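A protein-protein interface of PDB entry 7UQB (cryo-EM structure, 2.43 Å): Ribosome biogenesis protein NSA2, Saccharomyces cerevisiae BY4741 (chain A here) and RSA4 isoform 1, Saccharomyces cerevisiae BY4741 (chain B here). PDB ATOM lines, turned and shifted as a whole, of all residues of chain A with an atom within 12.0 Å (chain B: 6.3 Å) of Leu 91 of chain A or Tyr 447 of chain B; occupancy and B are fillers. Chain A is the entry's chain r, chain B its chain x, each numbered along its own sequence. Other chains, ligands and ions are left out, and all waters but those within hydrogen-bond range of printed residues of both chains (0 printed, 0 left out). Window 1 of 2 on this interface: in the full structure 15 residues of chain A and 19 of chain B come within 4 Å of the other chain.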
ATOM      1  N   ASP A  85     -34.483 -13.490  19.224  1.00  0.00           N
ATOM      2  CA  ASP A  85     -34.058 -14.149  17.995  1.00  0.00           C
ATOM      3  C   ASP A  85     -32.533 -14.156  17.875  1.00  0.00           C
ATOM      4  O   ASP A  85     -31.971 -14.961  17.130  1.00  0.00           O
ATOM      5  CB  ASP A  85     -34.687 -13.464  16.778  1.00  0.00           C
ATOM      6  CG  ASP A  85     -34.428 -14.215  15.484  1.00  0.00           C
ATOM      7  OD1 ASP A  85     -34.853 -15.386  15.377  1.00  0.00           O
ATOM      8  OD2 ASP A  85     -33.800 -13.634  14.573  1.00  0.00           O
ATOM      9  N   ALA A  86     -31.882 -13.262  18.624  1.00  0.00           N
ATOM     10  CA  ALA A  86     -30.421 -13.155  18.695  1.00  0.00           C
ATOM     11  C   ALA A  86     -29.818 -12.871  17.314  1.00  0.00           C
ATOM     12  O   ALA A  86     -29.166 -13.710  16.694  1.00  0.00           O
ATOM     13  CB  ALA A  86     -29.802 -14.407  19.329  1.00  0.00           C
ATOM     14  N   LEU A  87     -30.105 -11.650  16.825  1.00  0.00           N
ATOM     15  CA  LEU A  87     -29.560 -11.110  15.588  1.00  0.00           C
ATOM     16  C   LEU A  87     -28.249 -10.369  15.849  1.00  0.00           C
ATOM     17  O   LEU A  87     -28.036  -9.838  16.943  1.00  0.00           O
ATOM     18  CB  LEU A  87     -30.566 -10.164  14.938  1.00  0.00           C
ATOM     19  CG  LEU A  87     -31.848 -10.814  14.412  1.00  0.00           C
ATOM     20  CD1 LEU A  87     -32.902  -9.760  14.113  1.00  0.00           C
ATOM     21  CD2 LEU A  87     -31.554 -11.644  13.172  1.00  0.00           C
ATOM     22  N   PRO A  88     -27.340 -10.316  14.860  1.00  0.00           N
ATOM     23  CA  PRO A  88     -26.079  -9.582  15.050  1.00  0.00           C
ATOM     24  C   PRO A  88     -26.261  -8.073  15.002  1.00  0.00           C
ATOM     25  O   PRO A  88     -27.382  -7.584  14.839  1.00  0.00           O
ATOM     26  CB  PRO A  88     -25.206 -10.068  13.884  1.00  0.00           C
ATOM     27  CG  PRO A  88     -25.884 -11.282  13.352  1.00  0.00           C
ATOM     28  CD  PRO A  88     -27.337 -11.088  13.607  1.00  0.00           C
ATOM     29  N   THR A  89     -25.157  -7.331  15.137  1.00  0.00           N
ATOM     30  CA  THR A  89     -25.235  -5.873  15.183  1.00  0.00           C
ATOM     31  C   THR A  89     -25.686  -5.289  13.849  1.00  0.00           C
ATOM     32  O   THR A  89     -26.396  -4.278  13.820  1.00  0.00           O
ATOM     33  CB  THR A  89     -23.885  -5.278  15.582  1.00  0.00           C
ATOM     34  OG1 THR A  89     -22.896  -5.630  14.606  1.00  0.00           O
ATOM     35  CG2 THR A  89     -23.455  -5.791  16.943  1.00  0.00           C
ATOM     36  N   TYR A  90     -25.282  -5.897  12.739  1.00  0.00           N
ATOM     37  CA  TYR A  90     -25.635  -5.363  11.432  1.00  0.00           C
ATOM     38  C   TYR A  90     -27.029  -5.773  10.977  1.00  0.00           C
ATOM     39  O   TYR A  90     -27.459  -5.342   9.902  1.00  0.00           O
ATOM     40  CB  TYR A  90     -24.599  -5.786  10.385  1.00  0.00           C
ATOM     41  CG  TYR A  90     -24.373  -7.279  10.282  1.00  0.00           C
ATOM     42  CD1 TYR A  90     -25.147  -8.062   9.436  1.00  0.00           C
ATOM     43  CD2 TYR A  90     -23.376  -7.901  11.021  1.00  0.00           C
ATOM     44  CE1 TYR A  90     -24.940  -9.423   9.337  1.00  0.00           C
ATOM     45  CE2 TYR A  90     -23.163  -9.262  10.928  1.00  0.00           C
ATOM     46  CZ  TYR A  90     -23.947 -10.016  10.084  1.00  0.00           C
ATOM     47  OH  TYR A  90     -23.738 -11.371   9.990  1.00  0.00           O
ATOM     48  N   LEU A  91     -27.743  -6.586  11.758  1.00  0.00           N
ATOM     49  CA  LEU A  91     -29.078  -7.028  11.385  1.00  0.00           C
ATOM     50  C   LEU A  91     -30.182  -6.532  12.306  1.00  0.00           C
ATOM     51  O   LEU A  91     -31.347  -6.546  11.899  1.00  0.00           O
ATOM     52  CB  LEU A  91     -29.138  -8.560  11.318  1.00  0.00           C
ATOM     53  CG  LEU A  91     -28.615  -9.171  10.016  1.00  0.00           C
ATOM     54  CD1 LEU A  91     -28.745 -10.684  10.034  1.00  0.00           C
ATOM     55  CD2 LEU A  91     -29.344  -8.579   8.819  1.00  0.00           C
ATOM     56  N   LEU A  92     -29.864  -6.108  13.527  1.00  0.00           N
ATOM     57  CA  LEU A  92     -30.888  -5.474  14.343  1.00  0.00           C
ATOM     58  C   LEU A  92     -31.191  -4.081  13.800  1.00  0.00           C
ATOM     59  O   LEU A  92     -30.397  -3.489  13.062  1.00  0.00           O
ATOM     60  CB  LEU A  92     -30.471  -5.419  15.814  1.00  0.00           C
ATOM     61  CG  LEU A  92     -29.237  -4.647  16.276  1.00  0.00           C
ATOM     62  CD1 LEU A  92     -29.513  -3.160  16.393  1.00  0.00           C
ATOM     63  CD2 LEU A  92     -28.741  -5.211  17.599  1.00  0.00           C
ATOM     64  N   ASP A  93     -32.374  -3.576  14.161  1.00  0.00           N
ATOM     65  CA  ASP A  93     -33.002  -2.398  13.554  1.00  0.00           C
ATOM     66  C   ASP A  93     -33.300  -2.607  12.071  1.00  0.00           C
ATOM     67  O   ASP A  93     -33.494  -1.639  11.329  1.00  0.00           O
ATOM     68  CB  ASP A  93     -32.171  -1.125  13.760  1.00  0.00           C
ATOM     69  CG  ASP A  93     -32.139  -0.681  15.207  1.00  0.00           C
ATOM     70  OD1 ASP A  93     -33.177  -0.810  15.891  1.00  0.00           O
ATOM     71  OD2 ASP A  93     -31.078  -0.205  15.660  1.00  0.00           O
ATOM     72  N   ARG A  94     -33.332  -3.863  11.629  1.00  0.00           N
ATOM     73  CA  ARG A  94     -33.835  -4.245  10.318  1.00  0.00           C
ATOM     74  C   ARG A  94     -34.876  -5.333  10.526  1.00  0.00           C
ATOM     75  O   ARG A  94     -34.603  -6.332  11.198  1.00  0.00           O
ATOM     76  CB  ARG A  94     -32.719  -4.758   9.400  1.00  0.00           C
ATOM     77  CG  ARG A  94     -31.516  -3.844   9.253  1.00  0.00           C
ATOM     78  CD  ARG A  94     -30.632  -4.317   8.109  1.00  0.00           C
ATOM     79  NE  ARG A  94     -29.270  -3.803   8.197  1.00  0.00           N
ATOM     80  CZ  ARG A  94     -28.842  -2.698   7.601  1.00  0.00           C
ATOM     81  NH1 ARG A  94     -29.649  -1.953   6.864  1.00  0.00           N
ATOM     82  NH2 ARG A  94     -27.573  -2.334   7.747  1.00  0.00           N
ATOM     83  N   GLU A  95     -36.063  -5.142   9.961  1.00  0.00           N
ATOM     84  CA  GLU A  95     -37.141  -6.102  10.119  1.00  0.00           C
ATOM     85  C   GLU A  95     -37.118  -7.119   8.981  1.00  0.00           C
ATOM     86  O   GLU A  95     -36.285  -7.062   8.073  1.00  0.00           O
ATOM     87  CB  GLU A  95     -38.493  -5.389  10.187  1.00  0.00           C
ATOM     88  CG  GLU A  95     -38.722  -4.619  11.472  1.00  0.00           C
ATOM     89  CD  GLU A  95     -40.160  -4.174  11.621  1.00  0.00           C
ATOM     90  OE1 GLU A  95     -41.025  -4.719  10.904  1.00  0.00           O
ATOM     91  OE2 GLU A  95     -40.426  -3.281  12.453  1.00  0.00           O
ATOM     92  N   GLN A  96     -38.049  -8.066   9.045  1.00  0.00           N
ATOM     93  CA  GLN A  96     -38.170  -9.116   8.040  1.00  0.00           C
ATOM     94  C   GLN A  96     -38.571  -8.542   6.686  1.00  0.00           C
ATOM     95  O   GLN A  96     -39.741  -8.241   6.450  1.00  0.00           O
ATOM     96  CB  GLN A  96     -39.193 -10.165   8.485  1.00  0.00           C
ATOM     97  CG  GLN A  96     -38.871 -10.836   9.811  1.00  0.00           C
ATOM     98  CD  GLN A  96     -40.048 -11.613  10.369  1.00  0.00           C
ATOM     99  OE1 GLN A  96     -41.140 -11.597   9.802  1.00  0.00           O
ATOM    100  NE2 GLN A  96     -39.832 -12.295  11.488  1.00  0.00           N
ATOM    101  N   GLU A 188     -41.353 -21.920   6.104  1.00  0.00           N
ATOM    102  CA  GLU A 188     -40.304 -21.356   6.940  1.00  0.00           C
ATOM    103  C   GLU A 188     -40.013 -19.925   6.505  1.00  0.00           C
ATOM    104  O   GLU A 188     -40.027 -19.614   5.310  1.00  0.00           O
ATOM    105  CB  GLU A 188     -39.035 -22.206   6.859  1.00  0.00           C
ATOM    106  CG  GLU A 188     -37.880 -21.699   7.711  1.00  0.00           C
ATOM    107  CD  GLU A 188     -36.535 -22.257   7.277  1.00  0.00           C
ATOM    108  OE1 GLU A 188     -36.499 -23.063   6.323  1.00  0.00           O
ATOM    109  OE2 GLU A 188     -35.514 -21.884   7.890  1.00  0.00           O
ATOM    110  N   LEU A 189     -39.802 -19.052   7.495  1.00  0.00           N
ATOM    111  CA  LEU A 189     -39.466 -17.634   7.343  1.00  0.00           C
ATOM    112  C   LEU A 189     -40.648 -16.797   6.860  1.00  0.00           C
ATOM    113  O   LEU A 189     -40.542 -15.570   6.784  1.00  0.00           O
ATOM    114  CB  LEU A 189     -38.259 -17.437   6.415  1.00  0.00           C
ATOM    115  CG  LEU A 189     -36.911 -17.944   6.933  1.00  0.00           C
ATOM    116  CD1 LEU A 189     -35.790 -17.588   5.964  1.00  0.00           C
ATOM    117  CD2 LEU A 189     -36.625 -17.384   8.320  1.00  0.00           C
ATOM    118  N   VAL A 191     -42.560 -16.072   4.023  1.00  0.00           N
ATOM    119  CA  VAL A 191     -42.505 -15.140   2.906  1.00  0.00           C
ATOM    120  C   VAL A 191     -43.211 -15.748   1.701  1.00  0.00           C
ATOM    121  O   VAL A 191     -43.384 -16.965   1.593  1.00  0.00           O
ATOM    122  CB  VAL A 191     -41.057 -14.749   2.548  1.00  0.00           C
ATOM    123  CG1 VAL A 191     -40.455 -13.896   3.651  1.00  0.00           C
ATOM    124  CG2 VAL A 191     -40.215 -15.994   2.311  1.00  0.00           C
ATOM    125  N   GLU A 227     -34.392 -17.553  -6.476  1.00  0.00           N
ATOM    126  CA  GLU A 227     -34.313 -16.353  -5.655  1.00  0.00           C
ATOM    127  C   GLU A 227     -34.469 -16.630  -4.165  1.00  0.00           C
ATOM    128  O   GLU A 227     -34.260 -15.715  -3.360  1.00  0.00           O
ATOM    129  CB  GLU A 227     -35.362 -15.329  -6.103  1.00  0.00           C
ATOM    130  CG  GLU A 227     -36.741 -15.897  -6.404  1.00  0.00           C
ATOM    131  CD  GLU A 227     -36.883 -16.376  -7.841  1.00  0.00           C
ATOM    132  OE1 GLU A 227     -36.184 -17.341  -8.221  1.00  0.00           O
ATOM    133  OE2 GLU A 227     -37.686 -15.783  -8.592  1.00  0.00           O
ATOM    134  N   LEU A 228     -34.826 -17.853  -3.775  1.00  0.00           N
ATOM    135  CA  LEU A 228     -34.896 -18.206  -2.363  1.00  0.00           C
ATOM    136  C   LEU A 228     -33.532 -18.530  -1.766  1.00  0.00           C
ATOM    137  O   LEU A 228     -33.413 -18.587  -0.538  1.00  0.00           O
ATOM    138  CB  LEU A 228     -35.842 -19.392  -2.163  1.00  0.00           C
ATOM    139  CG  LEU A 228     -37.310 -19.148  -2.516  1.00  0.00           C
ATOM    140  CD1 LEU A 228     -38.141 -20.402  -2.290  1.00  0.00           C
ATOM    141  CD2 LEU A 228     -37.860 -17.988  -1.707  1.00  0.00           C
ATOM    142  N   GLY A 229     -32.514 -18.735  -2.594  1.00  0.00           N
ATOM    143  CA  GLY A 229     -31.162 -18.977  -2.117  1.00  0.00           C
ATOM    144  C   GLY A 229     -30.953 -20.267  -1.352  1.00  0.00           C
ATOM    145  O   GLY A 229     -30.213 -20.279  -0.362  1.00  0.00           O
ATOM    146  N   ASN B 405     -23.220  -4.017   2.931  1.00  0.00           N
ATOM    147  CA  ASN B 405     -23.240  -4.366   4.345  1.00  0.00           C
ATOM    148  C   ASN B 405     -21.850  -4.291   4.961  1.00  0.00           C
ATOM    149  O   ASN B 405     -21.671  -3.690   6.026  1.00  0.00           O
ATOM    150  CB  ASN B 405     -23.837  -5.758   4.539  1.00  0.00           C
ATOM    151  CG  ASN B 405     -24.053  -6.098   6.000  1.00  0.00           C
ATOM    152  OD1 ASN B 405     -24.817  -5.432   6.694  1.00  0.00           O
ATOM    153  ND2 ASN B 405     -23.387  -7.145   6.471  1.00  0.00           N
ATOM    154  N   HIS B 406     -20.851  -4.886   4.314  1.00  0.00           N
ATOM    155  CA  HIS B 406     -19.518  -4.942   4.898  1.00  0.00           C
ATOM    156  C   HIS B 406     -18.493  -4.413   3.910  1.00  0.00           C
ATOM    157  O   HIS B 406     -18.685  -4.487   2.696  1.00  0.00           O
ATOM    158  CB  HIS B 406     -19.151  -6.371   5.323  1.00  0.00           C
ATOM    159  CG  HIS B 406     -18.117  -6.434   6.403  1.00  0.00           C
ATOM    160  ND1 HIS B 406     -16.805  -6.771   6.159  1.00  0.00           N
ATOM    161  CD2 HIS B 406     -18.206  -6.205   7.735  1.00  0.00           C
ATOM    162  CE1 HIS B 406     -16.127  -6.746   7.293  1.00  0.00           C
ATOM    163  NE2 HIS B 406     -16.955  -6.407   8.264  1.00  0.00           N
ATOM    164  N   ALA B 419     -18.915  -6.350   0.524  1.00  0.00           N
ATOM    165  CA  ALA B 419     -19.897  -7.426   0.536  1.00  0.00           C
ATOM    166  C   ALA B 419     -21.279  -6.805   0.664  1.00  0.00           C
ATOM    167  O   ALA B 419     -21.543  -6.075   1.631  1.00  0.00           O
ATOM    168  CB  ALA B 419     -19.633  -8.395   1.687  1.00  0.00           C
ATOM    169  N   SER B 420     -22.157  -7.099  -0.299  1.00  0.00           N
ATOM    170  CA  SER B 420     -23.458  -6.447  -0.362  1.00  0.00           C
ATOM    171  C   SER B 420     -24.590  -7.456  -0.226  1.00  0.00           C
ATOM    172  O   SER B 420     -24.387  -8.672  -0.241  1.00  0.00           O
ATOM    173  CB  SER B 420     -23.614  -5.663  -1.667  1.00  0.00           C
ATOM    174  OG  SER B 420     -24.978  -5.432  -1.963  1.00  0.00           O
ATOM    175  N   PHE B 421     -25.804  -6.923  -0.097  1.00  0.00           N
ATOM    176  CA  PHE B 421     -27.010  -7.735  -0.017  1.00  0.00           C
ATOM    177  C   PHE B 421     -27.533  -8.154  -1.383  1.00  0.00           C
ATOM    178  O   PHE B 421     -28.539  -8.868  -1.448  1.00  0.00           O
ATOM    179  CB  PHE B 421     -28.111  -6.988   0.744  1.00  0.00           C
ATOM    180  CG  PHE B 421     -28.030  -7.132   2.240  1.00  0.00           C
ATOM    181  CD1 PHE B 421     -26.861  -7.549   2.855  1.00  0.00           C
ATOM    182  CD2 PHE B 421     -29.135  -6.862   3.031  1.00  0.00           C
ATOM    183  CE1 PHE B 421     -26.793  -7.682   4.226  1.00  0.00           C
ATOM    184  CE2 PHE B 421     -29.071  -6.996   4.405  1.00  0.00           C
ATOM    185  CZ  PHE B 421     -27.899  -7.405   5.003  1.00  0.00           C
ATOM    186  N   SER B 445     -27.652 -13.007   0.424  1.00  0.00           N
ATOM    187  CA  SER B 445     -26.900 -11.814   0.792  1.00  0.00           C
ATOM    188  C   SER B 445     -25.605 -12.180   1.507  1.00  0.00           C
ATOM    189  O   SER B 445     -25.563 -13.107   2.321  1.00  0.00           O
ATOM    190  CB  SER B 445     -27.750 -10.905   1.678  1.00  0.00           C
ATOM    191  OG  SER B 445     -28.032 -11.518   2.920  1.00  0.00           O
ATOM    192  N   VAL B 446     -24.541 -11.449   1.189  1.00  0.00           N
ATOM    193  CA  VAL B 446     -23.233 -11.670   1.793  1.00  0.00           C
ATOM    194  C   VAL B 446     -23.153 -10.829   3.060  1.00  0.00           C
ATOM    195  O   VAL B 446     -23.264  -9.600   3.007  1.00  0.00           O
ATOM    196  CB  VAL B 446     -22.100 -11.314   0.819  1.00  0.00           C
ATOM    197  CG1 VAL B 446     -20.781 -11.887   1.312  1.00  0.00           C
ATOM    198  CG2 VAL B 446     -22.421 -11.822  -0.576  1.00  0.00           C
ATOM    199  N   TYR B 447     -22.959 -11.490   4.199  1.00  0.00           N
ATOM    200  CA  TYR B 447     -23.032 -10.787   5.475  1.00  0.00           C
ATOM    201  C   TYR B 447     -21.708 -10.127   5.835  1.00  0.00           C
ATOM    202  O   TYR B 447     -21.679  -8.937   6.167  1.00  0.00           O
ATOM    203  CB  TYR B 447     -23.489 -11.745   6.575  1.00  0.00           C
ATOM    204  CG  TYR B 447     -24.985 -11.948   6.585  1.00  0.00           C
ATOM    205  CD1 TYR B 447     -25.838 -10.955   6.119  1.00  0.00           C
ATOM    206  CD2 TYR B 447     -25.546 -13.129   7.048  1.00  0.00           C
ATOM    207  CE1 TYR B 447     -27.203 -11.127   6.121  1.00  0.00           C
ATOM    208  CE2 TYR B 447     -26.916 -13.312   7.052  1.00  0.00           C
ATOM    209  CZ  TYR B 447     -27.739 -12.308   6.588  1.00  0.00           C
ATOM    210  OH  TYR B 447     -29.102 -12.480   6.590  1.00  0.00           O
ATOM    211  N   GLN B 448     -20.603 -10.868   5.775  1.00  0.00           N
ATOM    212  CA  GLN B 448     -19.308 -10.260   6.042  1.00  0.00           C
ATOM    213  C   GLN B 448     -18.197 -11.043   5.355  1.00  0.00           C
ATOM    214  O   GLN B 448     -18.394 -12.152   4.838  1.00  0.00           O
ATOM    215  CB  GLN B 448     -19.040 -10.127   7.548  1.00  0.00           C
ATOM    216  CG  GLN B 448     -18.454 -11.343   8.226  1.00  0.00           C
ATOM    217  CD  GLN B 448     -18.215 -11.100   9.703  1.00  0.00           C
ATOM    218  OE1 GLN B 448     -17.427 -11.795  10.342  1.00  0.00           O
ATOM    219  NE2 GLN B 448     -18.899 -10.103  10.252  1.00  0.00           N
ATOM    220  N   VAL B 449     -17.018 -10.418   5.357  1.00  0.00           N
ATOM    221  CA  VAL B 449     -15.867 -10.829   4.568  1.00  0.00           C
ATOM    222  C   VAL B 449     -14.617 -10.689   5.430  1.00  0.00           C
ATOM    223  O   VAL B 449     -14.619 -10.008   6.459  1.00  0.00           O
ATOM    224  CB  VAL B 449     -15.761  -9.981   3.277  1.00  0.00           C
ATOM    225  CG1 VAL B 449     -14.856  -8.765   3.483  1.00  0.00           C
ATOM    226  CG2 VAL B 449     -15.323 -10.822   2.106  1.00  0.00           C
ATOM    227  N   CYS B 461     -18.760 -15.069   4.213  1.00  0.00           N
ATOM    228  CA  CYS B 461     -19.852 -15.883   4.731  1.00  0.00           C
ATOM    229  C   CYS B 461     -21.172 -15.301   4.250  1.00  0.00           C
ATOM    230  O   CYS B 461     -21.329 -14.078   4.184  1.00  0.00           O
ATOM    231  CB  CYS B 461     -19.827 -15.951   6.261  1.00  0.00           C
ATOM    232  SG  CYS B 461     -20.122 -14.383   7.102  1.00  0.00           S
ATOM    233  N   SER B 462     -22.118 -16.164   3.891  1.00  0.00           N
ATOM    234  CA  SER B 462     -23.360 -15.652   3.332  1.00  0.00           C
ATOM    235  C   SER B 462     -24.573 -16.170   4.089  1.00  0.00           C
ATOM    236  O   SER B 462     -24.494 -17.085   4.913  1.00  0.00           O
ATOM    237  CB  SER B 462     -23.491 -16.003   1.847  1.00  0.00           C
ATOM    238  OG  SER B 462     -24.765 -15.642   1.344  1.00  0.00           O
ATOM    239  N   LYS B 463     -25.708 -15.537   3.787  1.00  0.00           N
ATOM    240  CA  LYS B 463     -27.018 -16.003   4.217  1.00  0.00           C
ATOM    241  C   LYS B 463     -27.369 -17.360   3.612  1.00  0.00           C
ATOM    242  O   LYS B 463     -28.231 -18.060   4.152  1.00  0.00           O
ATOM    243  CB  LYS B 463     -28.061 -14.942   3.845  1.00  0.00           C
ATOM    244  CG  LYS B 463     -29.497 -15.205   4.266  1.00  0.00           C
ATOM    245  CD  LYS B 463     -30.372 -14.018   3.895  1.00  0.00           C
ATOM    246  CE  LYS B 463     -31.828 -14.242   4.260  1.00  0.00           C
ATOM    247  NZ  LYS B 463     -32.488 -15.219   3.353  1.00  0.00           N
ATOM    248  N   GLU B 487     -27.918 -19.902   8.514  1.00  0.00           N
ATOM    249  CA  GLU B 487     -27.208 -18.697   8.102  1.00  0.00           C
ATOM    250  C   GLU B 487     -25.927 -18.518   8.905  1.00  0.00           C
ATOM    251  O   GLU B 487     -25.907 -18.712  10.123  1.00  0.00           O
ATOM    252  CB  GLU B 487     -28.094 -17.462   8.279  1.00  0.00           C
ATOM    253  CG  GLU B 487     -29.439 -17.525   7.583  1.00  0.00           C
ATOM    254  CD  GLU B 487     -30.189 -16.210   7.664  1.00  0.00           C
ATOM    255  OE1 GLU B 487     -29.532 -15.156   7.793  1.00  0.00           O
ATOM    256  OE2 GLU B 487     -31.436 -16.226   7.606  1.00  0.00           O
ATOM    257  N   VAL B 488     -24.854 -18.157   8.214  1.00  0.00           N
ATOM    258  CA  VAL B 488     -23.578 -17.871   8.857  1.00  0.00           C
ATOM    259  C   VAL B 488     -23.487 -16.372   9.090  1.00  0.00           C
ATOM    260  O   VAL B 488     -23.675 -15.576   8.162  1.00  0.00           O
ATOM    261  CB  VAL B 488     -22.402 -18.374   8.006  1.00  0.00           C
ATOM    262  CG1 VAL B 488     -21.114 -18.332   8.813  1.00  0.00           C
ATOM    263  CG2 VAL B 488     -22.677 -19.776   7.501  1.00  0.00           C
ATOM    264  N   TYR B 489     -23.209 -15.984  10.331  1.00  0.00           N
ATOM    265  CA  TYR B 489     -23.192 -14.580  10.712  1.00  0.00           C
ATOM    266  C   TYR B 489     -21.796 -13.986  10.797  1.00  0.00           C
ATOM    267  O   TYR B 489     -21.642 -12.779  10.586  1.00  0.00           O
ATOM    268  CB  TYR B 489     -23.888 -14.391  12.062  1.00  0.00           C
ATOM    269  CG  TYR B 489     -25.395 -14.435  11.995  1.00  0.00           C
ATOM    270  CD1 TYR B 489     -26.072 -14.039  10.850  1.00  0.00           C
ATOM    271  CD2 TYR B 489     -26.140 -14.862  13.081  1.00  0.00           C
ATOM    272  CE1 TYR B 489     -27.451 -14.075  10.788  1.00  0.00           C
ATOM    273  CE2 TYR B 489     -27.514 -14.898  13.032  1.00  0.00           C
ATOM    274  CZ  TYR B 489     -28.167 -14.509  11.883  1.00  0.00           C
ATOM    275  OH  TYR B 489     -29.540 -14.547  11.836  1.00  0.00           O
ATOM    276  N   THR B 490     -20.778 -14.786  11.102  1.00  0.00           N
ATOM    277  CA  THR B 490     -19.441 -14.244  11.290  1.00  0.00           C
ATOM    278  C   THR B 490     -18.392 -15.212  10.760  1.00  0.00           C
ATOM    279  O   THR B 490     -18.532 -16.433  10.891  1.00  0.00           O
ATOM    280  CB  THR B 490     -19.180 -13.922  12.771  1.00  0.00           C
ATOM    281  OG1 THR B 490     -17.811 -13.542  12.952  1.00  0.00           O
ATOM    282  CG2 THR B 490     -19.507 -15.120  13.656  1.00  0.00           C
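Among the printed residues, pairs that only touch across the chains: Leu 87 of chain A with Tyr 489 of chain B (3.8 Å), Pro 88 of chain A with Tyr 489 of chain B (3.5 Å), Tyr 90 of chain A with Asn 405 of chain B (3.6 Å), Tyr 90 of chain A with Tyr 447 of chain B (3.4 Å), Leu 91 of chain A with Tyr 447 of chain B (3.9 Å) and Leu 91 of chain A with Tyr 489 of chain B (3.7 Å).
The side-chain hydroxyl of Tyr 90 of chain A lies within hydrogen-bond range of the backbone carbonyl oxygen of Tyr 489 of chain B.
Among the printed residues, 7 pairs touch across the chains.
Of chain B, only Tyr 447 (3.9 Å) and Tyr 489 (3.7 Å) come within 4 Å of Leu 91 of chain A.
Tyr 447 of chain B touches two residues of chain A.
Asn 405 of chain B touches one residue of chain A.
Ser 445 of chain B touches none of the printed residues of chain A.
No residue of chain A comes within 4 Å of Val 446 of chain B.
Gln 448 of chain B touches none of the printed residues of chain A.
No residue of chain A comes within 4 Å of Val 449 of chain B.
No residue of chain A comes within 4 Å of Ser 462 of chain B.
No residue of chain A comes within 4 Å of Lys 463 of chain B.
No residue of chain A comes within 4 Å of Val 488 of chain B.
Tyr 489 of chain B touches just these residues of chain A: Leu 87, Pro 88, Tyr 90 and Leu 91.
Printed residues of chain B within 4 Å of Pro 88 of chain A: Tyr 489 (3.5 Å).
Of the printed residues of chain B, Tyr 90 of chain A touches Asn 405, Tyr 447 and Tyr 489.
Of the printed residues of chain B, Leu 87 of chain A touches Tyr 489.
Thr 89 of chain A touches none of the printed residues of chain B.
Glu 95 of chain A touches none of the printed residues of chain B.
The nearest residue of chain B that does not touch Leu 91 of chain A is Phe 421 of chain B (4.2 Å).
The nearest residue of chain A that does not touch Tyr 447 of chain B is Pro 88 of chain A (6.6 Å).
The backbone NH (N) of Asn 405 of chain B sits at hydrogen-bond distance from the backbone carbonyl oxygen (O) of Ala 419 of chain B (3.0 Å).
O of Cys 461 of chain B lies within hydrogen-bond range of N of Tyr 447 of chain B (3.1 Å).
O of Tyr 90 of chain A is in hydrogen-bond range of NE of Arg 94 of chain A (2.9 Å).
The side-chain carboxylate (OE1) of Glu 487 of chain B lies within hydrogen-bond range of the side-chain hydroxyl (OH) of Tyr 447 of chain B, 3.0 Å away.
The side-chain amide nitrogen (ND2) of Asn 405 of chain B is in hydrogen-bond range of the backbone carbonyl oxygen (O) of Tyr 447 of chain B (2.5 Å).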
